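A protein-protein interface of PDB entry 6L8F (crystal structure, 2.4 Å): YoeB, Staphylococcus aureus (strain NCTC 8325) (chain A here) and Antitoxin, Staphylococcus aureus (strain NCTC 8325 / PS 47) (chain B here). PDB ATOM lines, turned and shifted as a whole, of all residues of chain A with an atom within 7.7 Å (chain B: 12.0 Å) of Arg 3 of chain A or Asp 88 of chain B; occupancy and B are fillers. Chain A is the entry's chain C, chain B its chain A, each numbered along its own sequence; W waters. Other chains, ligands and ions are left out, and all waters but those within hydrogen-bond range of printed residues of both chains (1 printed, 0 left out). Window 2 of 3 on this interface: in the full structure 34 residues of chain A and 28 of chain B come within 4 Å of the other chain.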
ATOM      1  N   ALA A   2     -15.943  -6.576  14.480  1.00  0.00           N
ATOM      2  CA  ALA A   2     -16.478  -7.006  15.766  1.00  0.00           C
ATOM      3  C   ALA A   2     -15.625  -6.510  16.918  1.00  0.00           C
ATOM      4  O   ALA A   2     -16.026  -6.641  18.053  1.00  0.00           O
ATOM      5  CB  ALA A   2     -16.593  -8.512  15.831  1.00  0.00           C
ATOM      6  N   ARG A   3     -14.454  -5.948  16.645  1.00  0.00           N
ATOM      7  CA  ARG A   3     -13.612  -5.379  17.692  1.00  0.00           C
ATOM      8  C   ARG A   3     -13.302  -3.926  17.378  1.00  0.00           C
ATOM      9  O   ARG A   3     -13.003  -3.574  16.231  1.00  0.00           O
ATOM     10  CB  ARG A   3     -12.294  -6.134  17.859  1.00  0.00           C
ATOM     11  CG  ARG A   3     -12.426  -7.498  18.469  1.00  0.00           C
ATOM     12  CD  ARG A   3     -12.930  -7.436  19.876  1.00  0.00           C
ATOM     13  NE  ARG A   3     -13.144  -8.778  20.394  1.00  0.00           N
ATOM     14  CZ  ARG A   3     -12.222  -9.482  21.037  1.00  0.00           C
ATOM     15  NH1 ARG A   3     -12.501 -10.707  21.466  1.00  0.00           N
ATOM     16  NH2 ARG A   3     -11.021  -8.960  21.254  1.00  0.00           N
ATOM     17  N   LEU A   4     -13.372  -3.092  18.410  1.00  0.00           N
ATOM     18  CA  LEU A   4     -12.947  -1.701  18.339  1.00  0.00           C
ATOM     19  C   LEU A   4     -12.112  -1.406  19.567  1.00  0.00           C
ATOM     20  O   LEU A   4     -12.490  -1.789  20.678  1.00  0.00           O
ATOM     21  CB  LEU A   4     -14.131  -0.741  18.285  1.00  0.00           C
ATOM     22  CG  LEU A   4     -14.924  -0.685  16.991  1.00  0.00           C
ATOM     23  CD1 LEU A   4     -15.966   0.397  17.147  1.00  0.00           C
ATOM     24  CD2 LEU A   4     -14.011  -0.410  15.796  1.00  0.00           C
ATOM     25  N   ASN A   5     -10.976  -0.751  19.362  1.00  0.00           N
ATOM     26  CA  ASN A   5     -10.111  -0.340  20.458  1.00  0.00           C
ATOM     27  C   ASN A   5     -10.563   1.053  20.891  1.00  0.00           C
ATOM     28  O   ASN A   5     -10.383   2.029  20.152  1.00  0.00           O
ATOM     29  CB  ASN A   5      -8.651  -0.369  20.023  1.00  0.00           C
ATOM     30  CG  ASN A   5      -7.696  -0.293  21.189  1.00  0.00           C
ATOM     31  OD1 ASN A   5      -6.878   0.618  21.275  1.00  0.00           O
ATOM     32  ND2 ASN A   5      -7.802  -1.244  22.105  1.00  0.00           N
ATOM     33  N   ILE A   6     -11.187   1.131  22.069  1.00  0.00           N
ATOM     34  CA  ILE A   6     -11.878   2.326  22.550  1.00  0.00           C
ATOM     35  C   ILE A   6     -11.225   2.770  23.855  1.00  0.00           C
ATOM     36  O   ILE A   6     -10.942   1.938  24.721  1.00  0.00           O
ATOM     37  CB  ILE A   6     -13.380   2.053  22.767  1.00  0.00           C
ATOM     38  CG1 ILE A   6     -14.038   1.486  21.509  1.00  0.00           C
ATOM     39  CG2 ILE A   6     -14.109   3.300  23.220  1.00  0.00           C
ATOM     40  CD1 ILE A   6     -14.138   2.431  20.384  1.00  0.00           C
ATOM     41  N   TYR A  16     -20.571   1.734  31.193  1.00  0.00           N
ATOM     42  CA  TYR A  16     -20.595   0.743  30.122  1.00  0.00           C
ATOM     43  C   TYR A  16     -20.634  -0.669  30.698  1.00  0.00           C
ATOM     44  O   TYR A  16     -21.432  -1.500  30.252  1.00  0.00           O
ATOM     45  CB  TYR A  16     -19.381   0.920  29.197  1.00  0.00           C
ATOM     46  CG  TYR A  16     -19.391  -0.010  27.997  1.00  0.00           C
ATOM     47  CD1 TYR A  16     -20.121   0.308  26.861  1.00  0.00           C
ATOM     48  CD2 TYR A  16     -18.687  -1.213  28.009  1.00  0.00           C
ATOM     49  CE1 TYR A  16     -20.154  -0.539  25.769  1.00  0.00           C
ATOM     50  CE2 TYR A  16     -18.714  -2.075  26.917  1.00  0.00           C
ATOM     51  CZ  TYR A  16     -19.449  -1.729  25.805  1.00  0.00           C
ATOM     52  OH  TYR A  16     -19.483  -2.574  24.725  1.00  0.00           O
ATOM     53  N   GLN A  20     -23.566  -3.718  30.750  1.00  0.00           N
ATOM     54  CA  GLN A  20     -23.278  -5.065  30.269  1.00  0.00           C
ATOM     55  C   GLN A  20     -23.914  -6.134  31.143  1.00  0.00           C
ATOM     56  O   GLN A  20     -24.293  -7.197  30.636  1.00  0.00           O
ATOM     57  CB  GLN A  20     -21.772  -5.295  30.209  1.00  0.00           C
ATOM     58  CG  GLN A  20     -21.115  -5.014  28.890  1.00  0.00           C
ATOM     59  CD  GLN A  20     -19.611  -5.172  28.997  1.00  0.00           C
ATOM     60  OE1 GLN A  20     -18.995  -4.701  29.962  1.00  0.00           O
ATOM     61  NE2 GLN A  20     -19.010  -5.854  28.021  1.00  0.00           N
ATOM     62  N   VAL A  27     -26.241  -1.744  25.669  1.00  0.00           N
ATOM     63  CA  VAL A  27     -24.884  -1.969  25.158  1.00  0.00           C
ATOM     64  C   VAL A  27     -24.888  -2.086  23.642  1.00  0.00           C
ATOM     65  O   VAL A  27     -24.021  -1.523  22.956  1.00  0.00           O
ATOM     66  CB  VAL A  27     -24.262  -3.227  25.787  1.00  0.00           C
ATOM     67  CG1 VAL A  27     -22.872  -3.478  25.228  1.00  0.00           C
ATOM     68  CG2 VAL A  27     -24.165  -3.078  27.246  1.00  0.00           C
ATOM     69  N   LYS A  28     -25.873  -2.804  23.099  1.00  0.00           N
ATOM     70  CA  LYS A  28     -25.934  -3.038  21.659  1.00  0.00           C
ATOM     71  C   LYS A  28     -26.168  -1.738  20.899  1.00  0.00           C
ATOM     72  O   LYS A  28     -25.585  -1.521  19.831  1.00  0.00           O
ATOM     73  CB  LYS A  28     -27.030  -4.064  21.346  1.00  0.00           C
ATOM     74  CG  LYS A  28     -26.942  -4.643  19.945  1.00  0.00           C
ATOM     75  CD  LYS A  28     -28.012  -5.701  19.687  1.00  0.00           C
ATOM     76  CE  LYS A  28     -29.408  -5.106  19.798  1.00  0.00           C
ATOM     77  NZ  LYS A  28     -30.486  -6.095  19.530  1.00  0.00           N
ATOM     78  N   ASN A  31     -22.846   0.137  20.979  1.00  0.00           N
ATOM     79  CA  ASN A  31     -21.937  -0.509  20.033  1.00  0.00           C
ATOM     80  C   ASN A  31     -22.260  -0.128  18.590  1.00  0.00           C
ATOM     81  O   ASN A  31     -21.346   0.119  17.787  1.00  0.00           O
ATOM     82  CB  ASN A  31     -22.000  -2.030  20.219  1.00  0.00           C
ATOM     83  CG  ASN A  31     -21.402  -2.488  21.546  1.00  0.00           C
ATOM     84  OD1 ASN A  31     -20.730  -1.721  22.247  1.00  0.00           O
ATOM     85  ND2 ASN A  31     -21.635  -3.744  21.890  1.00  0.00           N
ATOM     86  N   GLU A  32     -23.552  -0.034  18.259  1.00  0.00           N
ATOM     87  CA  GLU A  32     -23.965   0.443  16.941  1.00  0.00           C
ATOM     88  C   GLU A  32     -23.536   1.882  16.694  1.00  0.00           C
ATOM     89  O   GLU A  32     -23.217   2.243  15.553  1.00  0.00           O
ATOM     90  CB  GLU A  32     -25.486   0.327  16.780  1.00  0.00           C
ATOM     91  CG  GLU A  32     -25.989  -1.095  16.631  1.00  0.00           C
ATOM     92  CD  GLU A  32     -25.229  -1.867  15.568  1.00  0.00           C
ATOM     93  OE1 GLU A  32     -25.197  -1.411  14.402  1.00  0.00           O
ATOM     94  OE2 GLU A  32     -24.646  -2.924  15.905  1.00  0.00           O
ATOM     95  N   LEU A  34     -20.812   3.286  18.102  1.00  0.00           N
ATOM     96  CA  LEU A  34     -19.359   3.203  17.974  1.00  0.00           C
ATOM     97  C   LEU A  34     -18.937   2.699  16.597  1.00  0.00           C
ATOM     98  O   LEU A  34     -18.015   3.256  15.986  1.00  0.00           O
ATOM     99  CB  LEU A  34     -18.806   2.283  19.055  1.00  0.00           C
ATOM    100  CG  LEU A  34     -18.888   2.794  20.483  1.00  0.00           C
ATOM    101  CD1 LEU A  34     -18.478   1.694  21.446  1.00  0.00           C
ATOM    102  CD2 LEU A  34     -17.986   4.019  20.622  1.00  0.00           C
ATOM    103  N   LYS A  35     -19.610   1.654  16.097  1.00  0.00           N
ATOM    104  CA  LYS A  35     -19.342   1.144  14.752  1.00  0.00           C
ATOM    105  C   LYS A  35     -19.614   2.205  13.695  1.00  0.00           C
ATOM    106  O   LYS A  35     -18.832   2.358  12.750  1.00  0.00           O
ATOM    107  CB  LYS A  35     -20.187  -0.100  14.483  1.00  0.00           C
ATOM    108  CG  LYS A  35     -19.507  -1.404  14.865  1.00  0.00           C
ATOM    109  CD  LYS A  35     -20.514  -2.508  15.143  1.00  0.00           C
ATOM    110  CE  LYS A  35     -21.473  -2.714  13.993  1.00  0.00           C
ATOM    111  NZ  LYS A  35     -22.572  -3.645  14.386  1.00  0.00           N
ATOM    112  N   ASP A  38     -16.753   4.758  13.792  1.00  0.00           N
ATOM    113  CA  ASP A  38     -15.556   4.207  13.175  1.00  0.00           C
ATOM    114  C   ASP A  38     -15.662   4.165  11.651  1.00  0.00           C
ATOM    115  O   ASP A  38     -14.672   4.423  10.962  1.00  0.00           O
ATOM    116  CB  ASP A  38     -15.294   2.818  13.746  1.00  0.00           C
ATOM    117  CG  ASP A  38     -14.152   2.112  13.049  1.00  0.00           C
ATOM    118  OD1 ASP A  38     -13.003   2.574  13.200  1.00  0.00           O
ATOM    119  OD2 ASP A  38     -14.402   1.099  12.356  1.00  0.00           O
ATOM    120  N   THR B  84      -8.482   1.792  28.316  1.00  0.00           N
ATOM    121  CA  THR B  84      -8.515   1.477  26.897  1.00  0.00           C
ATOM    122  C   THR B  84      -8.657  -0.034  26.741  1.00  0.00           C
ATOM    123  O   THR B  84      -7.845  -0.790  27.279  1.00  0.00           O
ATOM    124  CB  THR B  84      -7.252   1.994  26.199  1.00  0.00           C
ATOM    125  OG1 THR B  84      -7.149   3.419  26.378  1.00  0.00           O
ATOM    126  CG2 THR B  84      -7.298   1.689  24.722  1.00  0.00           C
ATOM    127  N   LYS B  85      -9.699  -0.475  26.039  1.00  0.00           N
ATOM    128  CA  LYS B  85      -9.947  -1.898  25.830  1.00  0.00           C
ATOM    129  C   LYS B  85     -10.418  -2.139  24.402  1.00  0.00           C
ATOM    130  O   LYS B  85     -11.038  -1.270  23.778  1.00  0.00           O
ATOM    131  CB  LYS B  85     -11.022  -2.478  26.780  1.00  0.00           C
ATOM    132  CG  LYS B  85     -10.705  -2.491  28.269  1.00  0.00           C
ATOM    133  CD  LYS B  85      -9.497  -3.359  28.604  1.00  0.00           C
ATOM    134  CE  LYS B  85      -9.183  -3.336  30.109  1.00  0.00           C
ATOM    135  NZ  LYS B  85      -7.798  -3.835  30.406  1.00  0.00           N
ATOM    136  N   ASP B  86     -10.112  -3.336  23.897  1.00  0.00           N
ATOM    137  CA  ASP B  86     -10.817  -3.879  22.741  1.00  0.00           C
ATOM    138  C   ASP B  86     -12.183  -4.360  23.182  1.00  0.00           C
ATOM    139  O   ASP B  86     -12.291  -5.196  24.082  1.00  0.00           O
ATOM    140  CB  ASP B  86     -10.056  -5.055  22.131  1.00  0.00           C
ATOM    141  CG  ASP B  86      -9.022  -4.623  21.143  1.00  0.00           C
ATOM    142  OD1 ASP B  86      -8.638  -3.440  21.184  1.00  0.00           O
ATOM    143  OD2 ASP B  86      -8.595  -5.462  20.320  1.00  0.00           O
ATOM    144  N   ILE B  87     -13.232  -3.846  22.564  1.00  0.00           N
ATOM    145  CA  ILE B  87     -14.562  -4.261  22.978  1.00  0.00           C
ATOM    146  C   ILE B  87     -15.291  -4.898  21.801  1.00  0.00           C
ATOM    147  O   ILE B  87     -15.059  -4.565  20.632  1.00  0.00           O
ATOM    148  CB  ILE B  87     -15.370  -3.090  23.577  1.00  0.00           C
ATOM    149  CG1 ILE B  87     -15.568  -1.991  22.559  1.00  0.00           C
ATOM    150  CG2 ILE B  87     -14.663  -2.503  24.813  1.00  0.00           C
ATOM    151  CD1 ILE B  87     -16.540  -0.985  23.037  1.00  0.00           C
ATOM    152  N   ASP B  88     -16.169  -5.846  22.125  1.00  0.00           N
ATOM    153  CA  ASP B  88     -16.986  -6.499  21.114  1.00  0.00           C
ATOM    154  C   ASP B  88     -18.127  -5.581  20.713  1.00  0.00           C
ATOM    155  O   ASP B  88     -18.834  -5.047  21.571  1.00  0.00           O
ATOM    156  CB  ASP B  88     -17.534  -7.833  21.620  1.00  0.00           C
ATOM    157  CG  ASP B  88     -16.442  -8.788  22.051  1.00  0.00           C
ATOM    158  OD1 ASP B  88     -16.511  -9.318  23.179  1.00  0.00           O
ATOM    159  OD2 ASP B  88     -15.503  -9.001  21.262  1.00  0.00           O
ATOM    160  N   VAL B  89     -18.304  -5.390  19.413  1.00  0.00           N
ATOM    161  CA  VAL B  89     -19.328  -4.476  18.931  1.00  0.00           C
ATOM    162  C   VAL B  89     -20.208  -5.177  17.906  1.00  0.00           C
ATOM    163  O   VAL B  89     -19.866  -6.265  17.428  1.00  0.00           O
ATOM    164  CB  VAL B  89     -18.700  -3.198  18.343  1.00  0.00           C
ATOM    165  CG1 VAL B  89     -18.180  -2.301  19.454  1.00  0.00           C
ATOM    166  CG2 VAL B  89     -17.575  -3.554  17.386  1.00  0.00           C
ATOM    167  OXT VAL B  89     -21.279  -4.672  17.548  1.00  0.00           O
HETATM  168  O   HOH W   1     -19.300  -5.148  24.281  1.00  0.00           O
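Hydrophobic or aromatic side chains of chain B within 4 Å of the printed part of chain A: Ile 87 and Val 89. Of the 14 printed residues of chain A, 9 touch a printed residue of chain B. Hydrophobic or aromatic side chains of chain A within 4 Å of the printed part of chain B: Leu 4, Ile 6, Tyr 16 and Leu 34. Among the printed residues, Asp or Glu carboxylates within 4 Å of a Lys or Arg side-chain nitrogen of the other chain: Arg 3 of chain A with Asp 88 of chain B.
Water W1 lies within hydrogen-bond range of the side-chain hydroxyl (OH) of Tyr 16 of chain A (2.6 Å) and the backbone carbonyl oxygen (O) of Asp 88 of chain B (2.8 Å).
The backbone carbonyl oxygen of Ala 2 of chain A sits at hydrogen-bond distance from the backbone NH of Val 89 of chain B, 2.9 Å away. The backbone carbonyl oxygen (O) of Asp 88 of chain B sits at hydrogen-bond distance from the side-chain amide nitrogen (ND2) of Asn 31 of chain A (3.1 Å). The backbone NH of Ile 6 of chain A sits at hydrogen-bond distance from the backbone carbonyl oxygen of Lys 85 of chain B. The side-chain carboxylate (OD2) of Asp 88 of chain B lies within salt-bridge range of the guanidinium group (NE) of Arg 3 of chain A, 2.5 Å away. The backbone carbonyl oxygen (O) of Ala 2 of chain A lies close to the backbone carbonyl oxygen (O) of Ile 87 of chain B, at 3.4 Å. The backbone NH of Ile 87 of chain B sits at hydrogen-bond distance from the backbone carbonyl oxygen of Leu 4 of chain A, 2.9 Å away. The backbone carbonyl oxygen (O) of Leu 4 of chain A sits close to the backbone carbonyl oxygen (O) of Lys 85 of chain B (3.5 Å). The chain-end carboxylate (OXT) of Val 89 of chain B is in salt-bridge range of the side-chain amino group (NZ) of Lys 35 of chain A (3.6 Å). The side-chain carboxylate (OD1) of Asp 86 of chain B is in hydrogen-bond range of the side-chain amide nitrogen (ND2) of Asn 5 of chain A, at 2.5 Å.
Ala 2 of chain A touches just these residues of chain B: Ile 87 (3.4 Å), Asp 88 (3.2 Å) and Val 89 (2.9 Å). Of the printed residues of chain B, Arg 3 of chain A touches Ile 87 and Asp 88. Of chain B, only Lys 85, Asp 86, Ile 87 and Val 89 come within 4 Å of Leu 4 of chain A. Of the printed residues of chain B, Asn 5 of chain A touches Thr 84 (3.6 Å), Lys 85 (3.6 Å) and Asp 86 (2.5 Å). Of the printed residues of chain B, Ile 6 of chain A touches Thr 84, Lys 85 and Ile 87. Asn 31 of chain A touches just these residues of chain B: Asp 88 (3.1 Å) and Val 89 (3.8 Å). Glu 32 of chain A touches none of the printed residues of chain B. Printed residues of chain B within 4 Å of Leu 34 of chain A: Ile 87 (3.7 Å). Asp 38 of chain A touches none of the printed residues of chain B. Of the printed residues of chain A, Thr 84 of chain B touches Asn 5 and Ile 6. Printed residues of chain A within 4 Å of Ile 87 of chain B: Ala 2 (3.4 Å), Arg 3 (3.4 Å), Leu 4 (2.9 Å), Ile 6 (3.8 Å), Tyr 16 (3.7 Å) and Leu 34 (3.7 Å). Asp 88 of chain B touches three residues of chain A. The nearest printed residue of chain B that does not touch Arg 3 of chain A is Val 89 of chain B (4.003 Å).
OH of Tyr 16 of chain A sits at hydrogen-bond distance from OD1 of Asn 31 of chain A (2.9 Å). The side-chain amide oxygen (OD1) of Asn 31 of chain A lies close to the backbone carbonyl oxygen (O) of Val 27 of chain A (3.4 Å). The side-chain amino group of Lys 35 of chain A is in salt-bridge range of the side-chain carboxylate of Glu 32 of chain A (2.7 Å).
Among the printed residues, merely in contact across the chains: Ala 2 of chain A with Asp 88 of chain B, Ile 6 of chain A with Thr 84 of chain B, Arg 3 of chain A with Ile 87 of chain B, Leu 4 of chain A with Asp 86 of chain B, Asn 5 of chain A with Lys 85 of chain B, Asn 5 of chain A with Thr 84 of chain B, Leu 34 of chain A with Ile 87 of chain B, Tyr 16 of chain A with Ile 87 of chain B, Asn 31 of chain A with Val 89 of chain B, Ile 6 of chain A with Ile 87 of chain B and Leu 4 of chain A with Val 89 of chain B.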
